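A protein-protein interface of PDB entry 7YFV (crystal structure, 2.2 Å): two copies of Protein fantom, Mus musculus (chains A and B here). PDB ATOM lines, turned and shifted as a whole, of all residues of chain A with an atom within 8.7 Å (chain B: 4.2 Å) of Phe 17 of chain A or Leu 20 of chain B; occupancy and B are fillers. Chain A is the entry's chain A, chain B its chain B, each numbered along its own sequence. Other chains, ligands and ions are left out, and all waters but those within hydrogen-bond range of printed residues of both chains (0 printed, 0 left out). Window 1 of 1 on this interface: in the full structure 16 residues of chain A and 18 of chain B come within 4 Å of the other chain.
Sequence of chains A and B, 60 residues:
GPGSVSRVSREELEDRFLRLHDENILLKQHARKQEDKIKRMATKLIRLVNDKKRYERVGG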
ATOM      1  N   VAL A   8      10.945  25.491 -22.115  1.00  0.00           N
ATOM      2  CA  VAL A   8      11.547  24.191 -22.377  1.00  0.00           C
ATOM      3  C   VAL A   8      11.725  24.057 -23.879  1.00  0.00           C
ATOM      4  O   VAL A   8      10.761  24.205 -24.639  1.00  0.00           O
ATOM      5  CB  VAL A   8      10.677  23.047 -21.831  1.00  0.00           C
ATOM      6  CG1 VAL A   8      11.351  21.700 -22.108  1.00  0.00           C
ATOM      7  CG2 VAL A   8      10.418  23.234 -20.342  1.00  0.00           C
ATOM      8  N   ARG A  10      12.242  22.333 -27.540  1.00  0.00           N
ATOM      9  CA  ARG A  10      11.536  21.218 -28.161  1.00  0.00           C
ATOM     10  C   ARG A  10      12.327  19.911 -28.090  1.00  0.00           C
ATOM     11  O   ARG A  10      11.745  18.842 -27.873  1.00  0.00           O
ATOM     12  CB  ARG A  10      11.206  21.549 -29.614  1.00  0.00           C
ATOM     13  CG  ARG A  10      10.510  20.413 -30.386  1.00  0.00           C
ATOM     14  CD  ARG A  10       9.059  20.233 -29.942  1.00  0.00           C
ATOM     15  NE  ARG A  10       8.475  18.983 -30.432  1.00  0.00           N
ATOM     16  CZ  ARG A  10       7.227  18.836 -30.869  1.00  0.00           C
ATOM     17  NH1 ARG A  10       6.401  19.874 -30.903  1.00  0.00           N
ATOM     18  NH2 ARG A  10       6.799  17.644 -31.271  1.00  0.00           N
ATOM     19  N   GLU A  11      13.647  19.967 -28.270  1.00  0.00           N
ATOM     20  CA  GLU A  11      14.411  18.726 -28.227  1.00  0.00           C
ATOM     21  C   GLU A  11      14.428  18.180 -26.790  1.00  0.00           C
ATOM     22  O   GLU A  11      14.342  16.963 -26.557  1.00  0.00           O
ATOM     23  CB  GLU A  11      15.884  18.935 -28.557  1.00  0.00           C
ATOM     24  CG  GLU A  11      16.573  17.608 -29.023  1.00  0.00           C
ATOM     25  CD  GLU A  11      18.005  17.378 -28.616  1.00  0.00           C
ATOM     26  OE1 GLU A  11      18.252  17.354 -27.388  1.00  0.00           O
ATOM     27  OE2 GLU A  11      18.883  17.775 -29.458  1.00  0.00           O
ATOM     28  N   GLU A  12      14.605  19.087 -25.818  1.00  0.00           N
ATOM     29  CA  GLU A  12      14.609  18.714 -24.406  1.00  0.00           C
ATOM     30  C   GLU A  12      13.263  18.150 -23.995  1.00  0.00           C
ATOM     31  O   GLU A  12      13.200  17.152 -23.268  1.00  0.00           O
ATOM     32  CB  GLU A  12      14.972  19.924 -23.542  1.00  0.00           C
ATOM     33  CG  GLU A  12      14.622  19.791 -22.054  1.00  0.00           C
ATOM     34  CD  GLU A  12      15.362  18.645 -21.381  1.00  0.00           C
ATOM     35  OE1 GLU A  12      16.417  18.215 -21.885  1.00  0.00           O
ATOM     36  OE2 GLU A  12      14.914  18.197 -20.316  1.00  0.00           O
ATOM     37  N   LEU A  13      12.172  18.773 -24.448  1.00  0.00           N
ATOM     38  CA  LEU A  13      10.854  18.255 -24.096  1.00  0.00           C
ATOM     39  C   LEU A  13      10.671  16.859 -24.667  1.00  0.00           C
ATOM     40  O   LEU A  13      10.167  15.957 -23.983  1.00  0.00           O
ATOM     41  CB  LEU A  13       9.765  19.195 -24.611  1.00  0.00           C
ATOM     42  CG  LEU A  13       8.303  18.796 -24.358  1.00  0.00           C
ATOM     43  CD1 LEU A  13       8.022  18.531 -22.897  1.00  0.00           C
ATOM     44  CD2 LEU A  13       7.373  19.876 -24.892  1.00  0.00           C
ATOM     45  N   GLU A  14      11.069  16.667 -25.927  1.00  0.00           N
ATOM     46  CA  GLU A  14      11.037  15.345 -26.547  1.00  0.00           C
ATOM     47  C   GLU A  14      11.945  14.358 -25.820  1.00  0.00           C
ATOM     48  O   GLU A  14      11.573  13.195 -25.622  1.00  0.00           O
ATOM     49  CB  GLU A  14      11.441  15.453 -28.020  1.00  0.00           C
ATOM     50  CG  GLU A  14      10.365  16.081 -28.904  1.00  0.00           C
ATOM     51  CD  GLU A  14      10.676  15.950 -30.390  1.00  0.00           C
ATOM     52  OE1 GLU A  14      11.692  15.310 -30.733  1.00  0.00           O
ATOM     53  OE2 GLU A  14       9.899  16.476 -31.216  1.00  0.00           O
ATOM     54  N   ASP A  15      13.149  14.798 -25.443  1.00  0.00           N
ATOM     55  CA  ASP A  15      14.088  13.946 -24.717  1.00  0.00           C
ATOM     56  C   ASP A  15      13.492  13.437 -23.405  1.00  0.00           C
ATOM     57  O   ASP A  15      13.459  12.227 -23.156  1.00  0.00           O
ATOM     58  CB  ASP A  15      15.372  14.734 -24.433  1.00  0.00           C
ATOM     59  CG  ASP A  15      16.566  13.850 -24.268  1.00  0.00           C
ATOM     60  OD1 ASP A  15      16.430  12.640 -24.549  1.00  0.00           O
ATOM     61  OD2 ASP A  15      17.629  14.354 -23.846  1.00  0.00           O
ATOM     62  N   ARG A  16      13.006  14.355 -22.560  1.00  0.00           N
ATOM     63  CA  ARG A  16      12.458  13.995 -21.246  1.00  0.00           C
ATOM     64  C   ARG A  16      11.226  13.124 -21.370  1.00  0.00           C
ATOM     65  O   ARG A  16      11.056  12.169 -20.603  1.00  0.00           O
ATOM     66  CB  ARG A  16      12.156  15.281 -20.491  1.00  0.00           C
ATOM     67  CG  ARG A  16      13.448  15.861 -20.172  1.00  0.00           C
ATOM     68  CD  ARG A  16      14.201  15.092 -19.105  1.00  0.00           C
ATOM     69  NE  ARG A  16      15.588  15.496 -19.172  1.00  0.00           N
ATOM     70  CZ  ARG A  16      16.521  14.745 -19.737  1.00  0.00           C
ATOM     71  NH1 ARG A  16      16.183  13.571 -20.191  1.00  0.00           N
ATOM     72  NH2 ARG A  16      17.771  15.159 -19.815  1.00  0.00           N
ATOM     73  N   PHE A  17      10.339  13.451 -22.312  1.00  0.00           N
ATOM     74  CA  PHE A  17       9.143  12.640 -22.495  1.00  0.00           C
ATOM     75  C   PHE A  17       9.520  11.185 -22.764  1.00  0.00           C
ATOM     76  O   PHE A  17       9.012  10.268 -22.111  1.00  0.00           O
ATOM     77  CB  PHE A  17       8.294  13.213 -23.632  1.00  0.00           C
ATOM     78  CG  PHE A  17       7.090  12.388 -23.944  1.00  0.00           C
ATOM     79  CD1 PHE A  17       5.937  12.518 -23.193  1.00  0.00           C
ATOM     80  CD2 PHE A  17       7.123  11.463 -24.972  1.00  0.00           C
ATOM     81  CE1 PHE A  17       4.827  11.753 -23.476  1.00  0.00           C
ATOM     82  CE2 PHE A  17       6.017  10.694 -25.256  1.00  0.00           C
ATOM     83  CZ  PHE A  17       4.871  10.842 -24.518  1.00  0.00           C
ATOM     84  N   LEU A  18      10.473  10.967 -23.675  1.00  0.00           N
ATOM     85  CA  LEU A  18      10.845   9.607 -24.053  1.00  0.00           C
ATOM     86  C   LEU A  18      11.406   8.836 -22.861  1.00  0.00           C
ATOM     87  O   LEU A  18      11.049   7.672 -22.648  1.00  0.00           O
ATOM     88  CB  LEU A  18      11.840   9.647 -25.220  1.00  0.00           C
ATOM     89  CG  LEU A  18      11.225  10.147 -26.537  1.00  0.00           C
ATOM     90  CD1 LEU A  18      12.289  10.472 -27.584  1.00  0.00           C
ATOM     91  CD2 LEU A  18      10.200   9.142 -27.090  1.00  0.00           C
ATOM     92  N   ARG A  19      12.264   9.477 -22.059  1.00  0.00           N
ATOM     93  CA  ARG A  19      12.860   8.806 -20.902  1.00  0.00           C
ATOM     94  C   ARG A  19      11.826   8.566 -19.825  1.00  0.00           C
ATOM     95  O   ARG A  19      11.863   7.524 -19.159  1.00  0.00           O
ATOM     96  CB  ARG A  19      14.071   9.616 -20.381  1.00  0.00           C
ATOM     97  CG  ARG A  19      15.249   9.243 -21.241  1.00  0.00           C
ATOM     98  CD  ARG A  19      14.958   9.936 -22.504  1.00  0.00           C
ATOM     99  NE  ARG A  19      15.835   9.796 -23.635  1.00  0.00           N
ATOM    100  CZ  ARG A  19      15.625   8.796 -24.486  1.00  0.00           C
ATOM    101  NH1 ARG A  19      14.628   7.942 -24.256  1.00  0.00           N
ATOM    102  NH2 ARG A  19      16.364   8.653 -25.568  1.00  0.00           N
ATOM    103  N   LEU A  20      10.872   9.484 -19.678  1.00  0.00           N
ATOM    104  CA  LEU A  20       9.714   9.205 -18.841  1.00  0.00           C
ATOM    105  C   LEU A  20       8.888   8.063 -19.406  1.00  0.00           C
ATOM    106  O   LEU A  20       8.406   7.204 -18.659  1.00  0.00           O
ATOM    107  CB  LEU A  20       8.841  10.447 -18.722  1.00  0.00           C
ATOM    108  CG  LEU A  20       9.005  11.262 -17.455  1.00  0.00           C
ATOM    109  CD1 LEU A  20       8.043  12.428 -17.513  1.00  0.00           C
ATOM    110  CD2 LEU A  20       8.728  10.377 -16.251  1.00  0.00           C
ATOM    111  N   HIS A  21       8.731   8.025 -20.727  1.00  0.00           N
ATOM    112  CA  HIS A  21       7.968   6.944 -21.340  1.00  0.00           C
ATOM    113  C   HIS A  21       8.661   5.598 -21.154  1.00  0.00           C
ATOM    114  O   HIS A  21       8.027   4.615 -20.752  1.00  0.00           O
ATOM    115  CB  HIS A  21       7.748   7.233 -22.823  1.00  0.00           C
ATOM    116  CG  HIS A  21       6.957   6.172 -23.519  1.00  0.00           C
ATOM    117  ND1 HIS A  21       7.545   5.139 -24.219  1.00  0.00           N
ATOM    118  CD2 HIS A  21       5.621   5.961 -23.589  1.00  0.00           C
ATOM    119  CE1 HIS A  21       6.603   4.348 -24.704  1.00  0.00           C
ATOM    120  NE2 HIS A  21       5.428   4.825 -24.337  1.00  0.00           N
ATOM    121  N   ASP A  22       9.968   5.540 -21.429  1.00  0.00           N
ATOM    122  CA  ASP A  22      10.707   4.288 -21.287  1.00  0.00           C
ATOM    123  C   ASP A  22      10.699   3.822 -19.841  1.00  0.00           C
ATOM    124  O   ASP A  22      10.553   2.626 -19.566  1.00  0.00           O
ATOM    125  CB  ASP A  22      12.148   4.454 -21.788  1.00  0.00           C
ATOM    126  CG  ASP A  22      12.239   4.621 -23.312  1.00  0.00           C
ATOM    127  OD1 ASP A  22      11.272   4.282 -24.028  1.00  0.00           O
ATOM    128  OD2 ASP A  22      13.289   5.095 -23.798  1.00  0.00           O
ATOM    129  N   GLU A  23      10.847   4.758 -18.900  1.00  0.00           N
ATOM    130  CA  GLU A  23      10.792   4.386 -17.489  1.00  0.00           C
ATOM    131  C   GLU A  23       9.393   3.913 -17.109  1.00  0.00           C
ATOM    132  O   GLU A  23       9.242   2.936 -16.365  1.00  0.00           O
ATOM    133  CB  GLU A  23      11.228   5.564 -16.616  1.00  0.00           C
ATOM    134  CG  GLU A  23      10.939   5.376 -15.131  1.00  0.00           C
ATOM    135  CD  GLU A  23      11.416   6.547 -14.289  1.00  0.00           C
ATOM    136  OE1 GLU A  23      12.626   6.860 -14.322  1.00  0.00           O
ATOM    137  OE2 GLU A  23      10.573   7.161 -13.603  1.00  0.00           O
ATOM    138  N   ASN A  24       8.359   4.577 -17.638  1.00  0.00           N
ATOM    139  CA  ASN A  24       6.982   4.172 -17.367  1.00  0.00           C
ATOM    140  C   ASN A  24       6.732   2.751 -17.858  1.00  0.00           C
ATOM    141  O   ASN A  24       6.068   1.955 -17.184  1.00  0.00           O
ATOM    142  CB  ASN A  24       6.022   5.178 -18.014  1.00  0.00           C
ATOM    143  CG  ASN A  24       4.587   4.680 -18.105  1.00  0.00           C
ATOM    144  OD1 ASN A  24       4.262   3.787 -18.892  1.00  0.00           O
ATOM    145  ND2 ASN A  24       3.715   5.276 -17.303  1.00  0.00           N
ATOM    146  N   ILE A  25       7.258   2.415 -19.036  1.00  0.00           N
ATOM    147  CA  ILE A  25       7.110   1.066 -19.580  1.00  0.00           C
ATOM    148  C   ILE A  25       7.754   0.040 -18.658  1.00  0.00           C
ATOM    149  O   ILE A  25       7.198  -1.029 -18.396  1.00  0.00           O
ATOM    150  CB  ILE A  25       7.708   0.981 -20.991  1.00  0.00           C
ATOM    151  CG1 ILE A  25       7.089   2.026 -21.894  1.00  0.00           C
ATOM    152  CG2 ILE A  25       7.452  -0.366 -21.563  1.00  0.00           C
ATOM    153  CD1 ILE A  25       5.631   1.889 -21.993  1.00  0.00           C
ATOM    154  N   LEU A  27       8.463   0.315 -15.444  1.00  0.00           N
ATOM    155  CA  LEU A  27       7.725   0.214 -14.187  1.00  0.00           C
ATOM    156  C   LEU A  27       6.497  -0.681 -14.338  1.00  0.00           C
ATOM    157  O   LEU A  27       6.195  -1.490 -13.454  1.00  0.00           O
ATOM    158  CB  LEU A  27       7.309   1.607 -13.704  1.00  0.00           C
ATOM    159  CG  LEU A  27       8.412   2.488 -13.121  1.00  0.00           C
ATOM    160  CD1 LEU A  27       7.870   3.883 -12.840  1.00  0.00           C
ATOM    161  CD2 LEU A  27       8.983   1.853 -11.854  1.00  0.00           C
ATOM    162  N   LYS A  28       5.769  -0.550 -15.452  1.00  0.00           N
ATOM    163  CA  LYS A  28       4.570  -1.363 -15.619  1.00  0.00           C
ATOM    164  C   LYS A  28       4.921  -2.834 -15.821  1.00  0.00           C
ATOM    165  O   LYS A  28       4.258  -3.718 -15.269  1.00  0.00           O
ATOM    166  CB  LYS A  28       3.744  -0.843 -16.790  1.00  0.00           C
ATOM    167  CG  LYS A  28       3.059   0.486 -16.521  1.00  0.00           C
ATOM    168  CD  LYS A  28       2.461   1.042 -17.800  1.00  0.00           C
ATOM    169  CE  LYS A  28       1.470   2.149 -17.508  1.00  0.00           C
ATOM    170  NZ  LYS A  28       0.947   2.750 -18.767  1.00  0.00           N
ATOM    171  N   LEU B  13       2.243  17.692 -26.593  1.00  0.00           N
ATOM    172  CA  LEU B  13       3.448  17.105 -26.020  1.00  0.00           C
ATOM    173  C   LEU B  13       3.656  17.564 -24.583  1.00  0.00           C
ATOM    174  O   LEU B  13       3.994  16.755 -23.711  1.00  0.00           O
ATOM    175  CB  LEU B  13       4.665  17.456 -26.872  1.00  0.00           C
ATOM    176  CG  LEU B  13       5.941  16.741 -26.428  1.00  0.00           C
ATOM    177  CD1 LEU B  13       5.666  15.253 -26.248  1.00  0.00           C
ATOM    178  CD2 LEU B  13       7.066  16.973 -27.422  1.00  0.00           C
ATOM    179  N   ARG B  16       1.081  15.782 -22.510  1.00  0.00           N
ATOM    180  CA  ARG B  16       1.425  14.376 -22.332  1.00  0.00           C
ATOM    181  C   ARG B  16       2.573  14.212 -21.347  1.00  0.00           C
ATOM    182  O   ARG B  16       2.577  13.273 -20.544  1.00  0.00           O
ATOM    183  CB  ARG B  16       1.790  13.746 -23.675  1.00  0.00           C
ATOM    184  CG  ARG B  16       0.618  13.525 -24.613  1.00  0.00           C
ATOM    185  CD  ARG B  16       0.871  12.312 -25.481  1.00  0.00           C
ATOM    186  NE  ARG B  16       0.324  12.462 -26.822  1.00  0.00           N
ATOM    187  CZ  ARG B  16       0.873  11.925 -27.909  1.00  0.00           C
ATOM    188  NH1 ARG B  16       1.985  11.205 -27.804  1.00  0.00           N
ATOM    189  NH2 ARG B  16       0.315  12.107 -29.098  1.00  0.00           N
ATOM    190  N   PHE B  17       3.564  15.104 -21.404  1.00  0.00           N
ATOM    191  CA  PHE B  17       4.668  15.030 -20.454  1.00  0.00           C
ATOM    192  C   PHE B  17       4.168  15.227 -19.031  1.00  0.00           C
ATOM    193  O   PHE B  17       4.581  14.514 -18.113  1.00  0.00           O
ATOM    194  CB  PHE B  17       5.728  16.076 -20.798  1.00  0.00           C
ATOM    195  CG  PHE B  17       6.801  16.214 -19.752  1.00  0.00           C
ATOM    196  CD1 PHE B  17       7.880  15.350 -19.729  1.00  0.00           C
ATOM    197  CD2 PHE B  17       6.720  17.199 -18.788  1.00  0.00           C
ATOM    198  CE1 PHE B  17       8.859  15.473 -18.764  1.00  0.00           C
ATOM    199  CE2 PHE B  17       7.695  17.324 -17.824  1.00  0.00           C
ATOM    200  CZ  PHE B  17       8.761  16.459 -17.809  1.00  0.00           C
ATOM    201  N   LEU B  18       3.287  16.204 -18.827  1.00  0.00           N
ATOM    202  CA  LEU B  18       2.781  16.465 -17.486  1.00  0.00           C
ATOM    203  C   LEU B  18       2.016  15.262 -16.945  1.00  0.00           C
ATOM    204  O   LEU B  18       2.237  14.834 -15.807  1.00  0.00           O
ATOM    205  CB  LEU B  18       1.896  17.707 -17.509  1.00  0.00           C
ATOM    206  CG  LEU B  18       2.708  19.000 -17.649  1.00  0.00           C
ATOM    207  CD1 LEU B  18       1.797  20.217 -17.758  1.00  0.00           C
ATOM    208  CD2 LEU B  18       3.704  19.153 -16.505  1.00  0.00           C
ATOM    209  N   ARG B  19       1.123  14.690 -17.757  1.00  0.00           N
ATOM    210  CA  ARG B  19       0.362  13.534 -17.293  1.00  0.00           C
ATOM    211  C   ARG B  19       1.259  12.313 -17.120  1.00  0.00           C
ATOM    212  O   ARG B  19       1.036  11.508 -16.206  1.00  0.00           O
ATOM    213  CB  ARG B  19      -0.783  13.231 -18.265  1.00  0.00           C
ATOM    214  CG  ARG B  19      -1.817  14.350 -18.380  1.00  0.00           C
ATOM    215  CD  ARG B  19      -2.805  14.085 -19.513  1.00  0.00           C
ATOM    216  NE  ARG B  19      -3.159  15.296 -20.250  1.00  0.00           N
ATOM    217  CZ  ARG B  19      -4.045  16.198 -19.838  1.00  0.00           C
ATOM    218  NH1 ARG B  19      -4.687  16.034 -18.689  1.00  0.00           N
ATOM    219  NH2 ARG B  19      -4.294  17.265 -20.584  1.00  0.00           N
ATOM    220  N   LEU B  20       2.274  12.162 -17.967  1.00  0.00           N
ATOM    221  CA  LEU B  20       3.158  11.009 -17.846  1.00  0.00           C
ATOM    222  C   LEU B  20       3.987  11.085 -16.571  1.00  0.00           C
ATOM    223  O   LEU B  20       4.254  10.058 -15.937  1.00  0.00           O
ATOM    224  CB  LEU B  20       4.063  10.911 -19.077  1.00  0.00           C
ATOM    225  CG  LEU B  20       4.804   9.596 -19.296  1.00  0.00           C
ATOM    226  CD1 LEU B  20       3.856   8.428 -19.128  1.00  0.00           C
ATOM    227  CD2 LEU B  20       5.433   9.563 -20.677  1.00  0.00           C
ATOM    228  N   HIS B  21       4.423  12.285 -16.182  1.00  0.00           N
ATOM    229  CA  HIS B  21       5.173  12.408 -14.935  1.00  0.00           C
ATOM    230  C   HIS B  21       4.304  12.040 -13.737  1.00  0.00           C
ATOM    231  O   HIS B  21       4.736  11.301 -12.848  1.00  0.00           O
ATOM    232  CB  HIS B  21       5.730  13.824 -14.778  1.00  0.00           C
ATOM    233  CG  HIS B  21       6.653  13.971 -13.608  1.00  0.00           C
ATOM    234  ND1 HIS B  21       6.631  15.065 -12.771  1.00  0.00           N
ATOM    235  CD2 HIS B  21       7.612  13.145 -13.124  1.00  0.00           C
ATOM    236  CE1 HIS B  21       7.540  14.910 -11.824  1.00  0.00           C
ATOM    237  NE2 HIS B  21       8.150  13.753 -12.016  1.00  0.00           N
ATOM    238  N   ASP B  22       3.066  12.548 -13.699  1.00  0.00           N
ATOM    239  CA  ASP B  22       2.170  12.228 -12.586  1.00  0.00           C
ATOM    240  C   ASP B  22       1.861  10.739 -12.545  1.00  0.00           C
ATOM    241  O   ASP B  22       1.723  10.154 -11.466  1.00  0.00           O
ATOM    242  CB  ASP B  22       0.883  13.050 -12.687  1.00  0.00           C
ATOM    243  CG  ASP B  22       1.091  14.507 -12.300  1.00  0.00           C
ATOM    244  OD1 ASP B  22       2.186  14.848 -11.803  1.00  0.00           O
ATOM    245  OD2 ASP B  22       0.173  15.319 -12.520  1.00  0.00           O
ATOM    246  N   GLU B  23       1.711  10.115 -13.710  1.00  0.00           N
ATOM    247  CA  GLU B  23       1.481   8.676 -13.726  1.00  0.00           C
ATOM    248  C   GLU B  23       2.701   7.928 -13.192  1.00  0.00           C
ATOM    249  O   GLU B  23       2.562   6.957 -12.441  1.00  0.00           O
ATOM    250  CB  GLU B  23       1.136   8.229 -15.145  1.00  0.00           C
ATOM    251  CG  GLU B  23       1.355   6.758 -15.417  1.00  0.00           C
ATOM    252  CD  GLU B  23       0.744   6.334 -16.740  1.00  0.00           C
ATOM    253  OE1 GLU B  23       0.711   5.121 -17.005  1.00  0.00           O
ATOM    254  OE2 GLU B  23       0.300   7.213 -17.515  1.00  0.00           O
ATOM    255  N   ASN B  24       3.908   8.384 -13.543  1.00  0.00           N
ATOM    256  CA  ASN B  24       5.111   7.727 -13.036  1.00  0.00           C
ATOM    257  C   ASN B  24       5.212   7.855 -11.517  1.00  0.00           C
ATOM    258  O   ASN B  24       5.651   6.919 -10.837  1.00  0.00           O
ATOM    259  CB  ASN B  24       6.356   8.305 -13.714  1.00  0.00           C
ATOM    260  CG  ASN B  24       6.724   7.562 -14.997  1.00  0.00           C
ATOM    261  OD1 ASN B  24       5.856   7.149 -15.770  1.00  0.00           O
ATOM    262  ND2 ASN B  24       8.018   7.381 -15.218  1.00  0.00           N
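The side-chain amide nitrogen of Asn 24 of chain A is in hydrogen-bond range of the side-chain carboxylate of Glu 23 of chain B, 3.0 Å away. The side-chain amide nitrogen of Asn 24 of chain B is in hydrogen-bond range of the side-chain carboxylate of Glu 23 of chain A, 3.0 Å away. NZ of Lys 28 of chain A lies within salt-bridge range of OE1 of Glu 23 of chain B. The side-chain amide oxygen (OD1) of Asn 24 of chain B sits close to the side-chain amide nitrogen (ND2) of Asn 24 of chain A (3.2 Å). The backbone carbonyl oxygen of Leu 20 of chain A lies close to the side-chain amide nitrogen of Asn 24 of chain B (3.5 Å).
The backbone carbonyl oxygen of Leu 20 of chain B lies close to the side-chain amide oxygen of Asn 24 of chain B (3.3 Å). OD1 of Asn 24 of chain A lies close to NZ of Lys 28 of chain A, 3.5 Å away. OE2 of Glu 14 of chain A is in salt-bridge range of NE of Arg 10 of chain A (3.0 Å). NE of Arg 16 of chain A lies within salt-bridge range of OE2 of Glu 12 of chain A, 3.0 Å away.
Leu 13 of chain A touches Phe 17 of chain B. CD2 of Leu 13 of chain B touches CG of Glu 14 of chain A (3.7 Å). Phe 17 of chain A touches Leu 13 of chain B (CG to CD1, 3.9 Å). Phe 17 of chain A touches Arg 16 of chain B (CE1 to CB, 3.6 Å). CD1 of Phe 17 of chain A touches CA of Phe 17 of chain B (3.9 Å). Phe 17 of chain A touches Leu 20 of chain B. CD1 of Leu 20 of chain A touches CE1 of Phe 17 of chain B, at 3.4 Å. Leu 20 of chain A touches His 21 of chain B. His 21 of chain A touches Leu 20 of chain B. Leu 20 of chain B touches Asn 24 of chain A (CD1 to ND2, 3.6 Å).
Printed residues of chain B within 4 Å of Arg 10 of chain A: Leu 13. Of the printed residues of chain B, Glu 14 of chain A touches Leu 13. Phe 17 of chain A touches just these residues of chain B: Leu 13 (3.9 Å), Arg 16 (3.6 Å), Phe 17 (3.9 Å) and Leu 20 (3.6 Å). Printed residues of chain B within 4 Å of Leu 20 of chain A: Phe 17 (3.4 Å), Leu 20 (3.98 Å), His 21 (3.8 Å) and Asn 24 (3.2 Å). Leu 20 of chain B touches just these residues of chain A: Phe 17 (3.6 Å), Leu 20 (3.98 Å), His 21 (3.6 Å) and Asn 24 (3.6 Å). Asp 22 of chain B touches none of the printed residues of chain A.
Of the 10 printed residues of chain B, 7 touch a printed residue of chain A. Hydrophobic or aromatic side chains of chain B that line the printed part of chain A: Leu 13, Phe 17, Leu 20 and His 21.
Leu 13 of chain A touches its own counterpart, Leu 13 of chain B. Phe 17 of chain A touches Leu 20 of chain B, and with the chains exchanged Leu 20 of chain A touches Phe 17 of chain B. Leu 20 of chain A touches His 21 of chain B, and with the chains exchanged His 21 of chain A touches Leu 20 of chain B. Glu 23 of chain A touches Asn 24 of chain B, and with the chains exchanged Asn 24 of chain A touches Glu 23 of chain B. Positions printed for both chains: 13, 16, 17, 18, 19, 20, 21, 22, 23 and 24.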
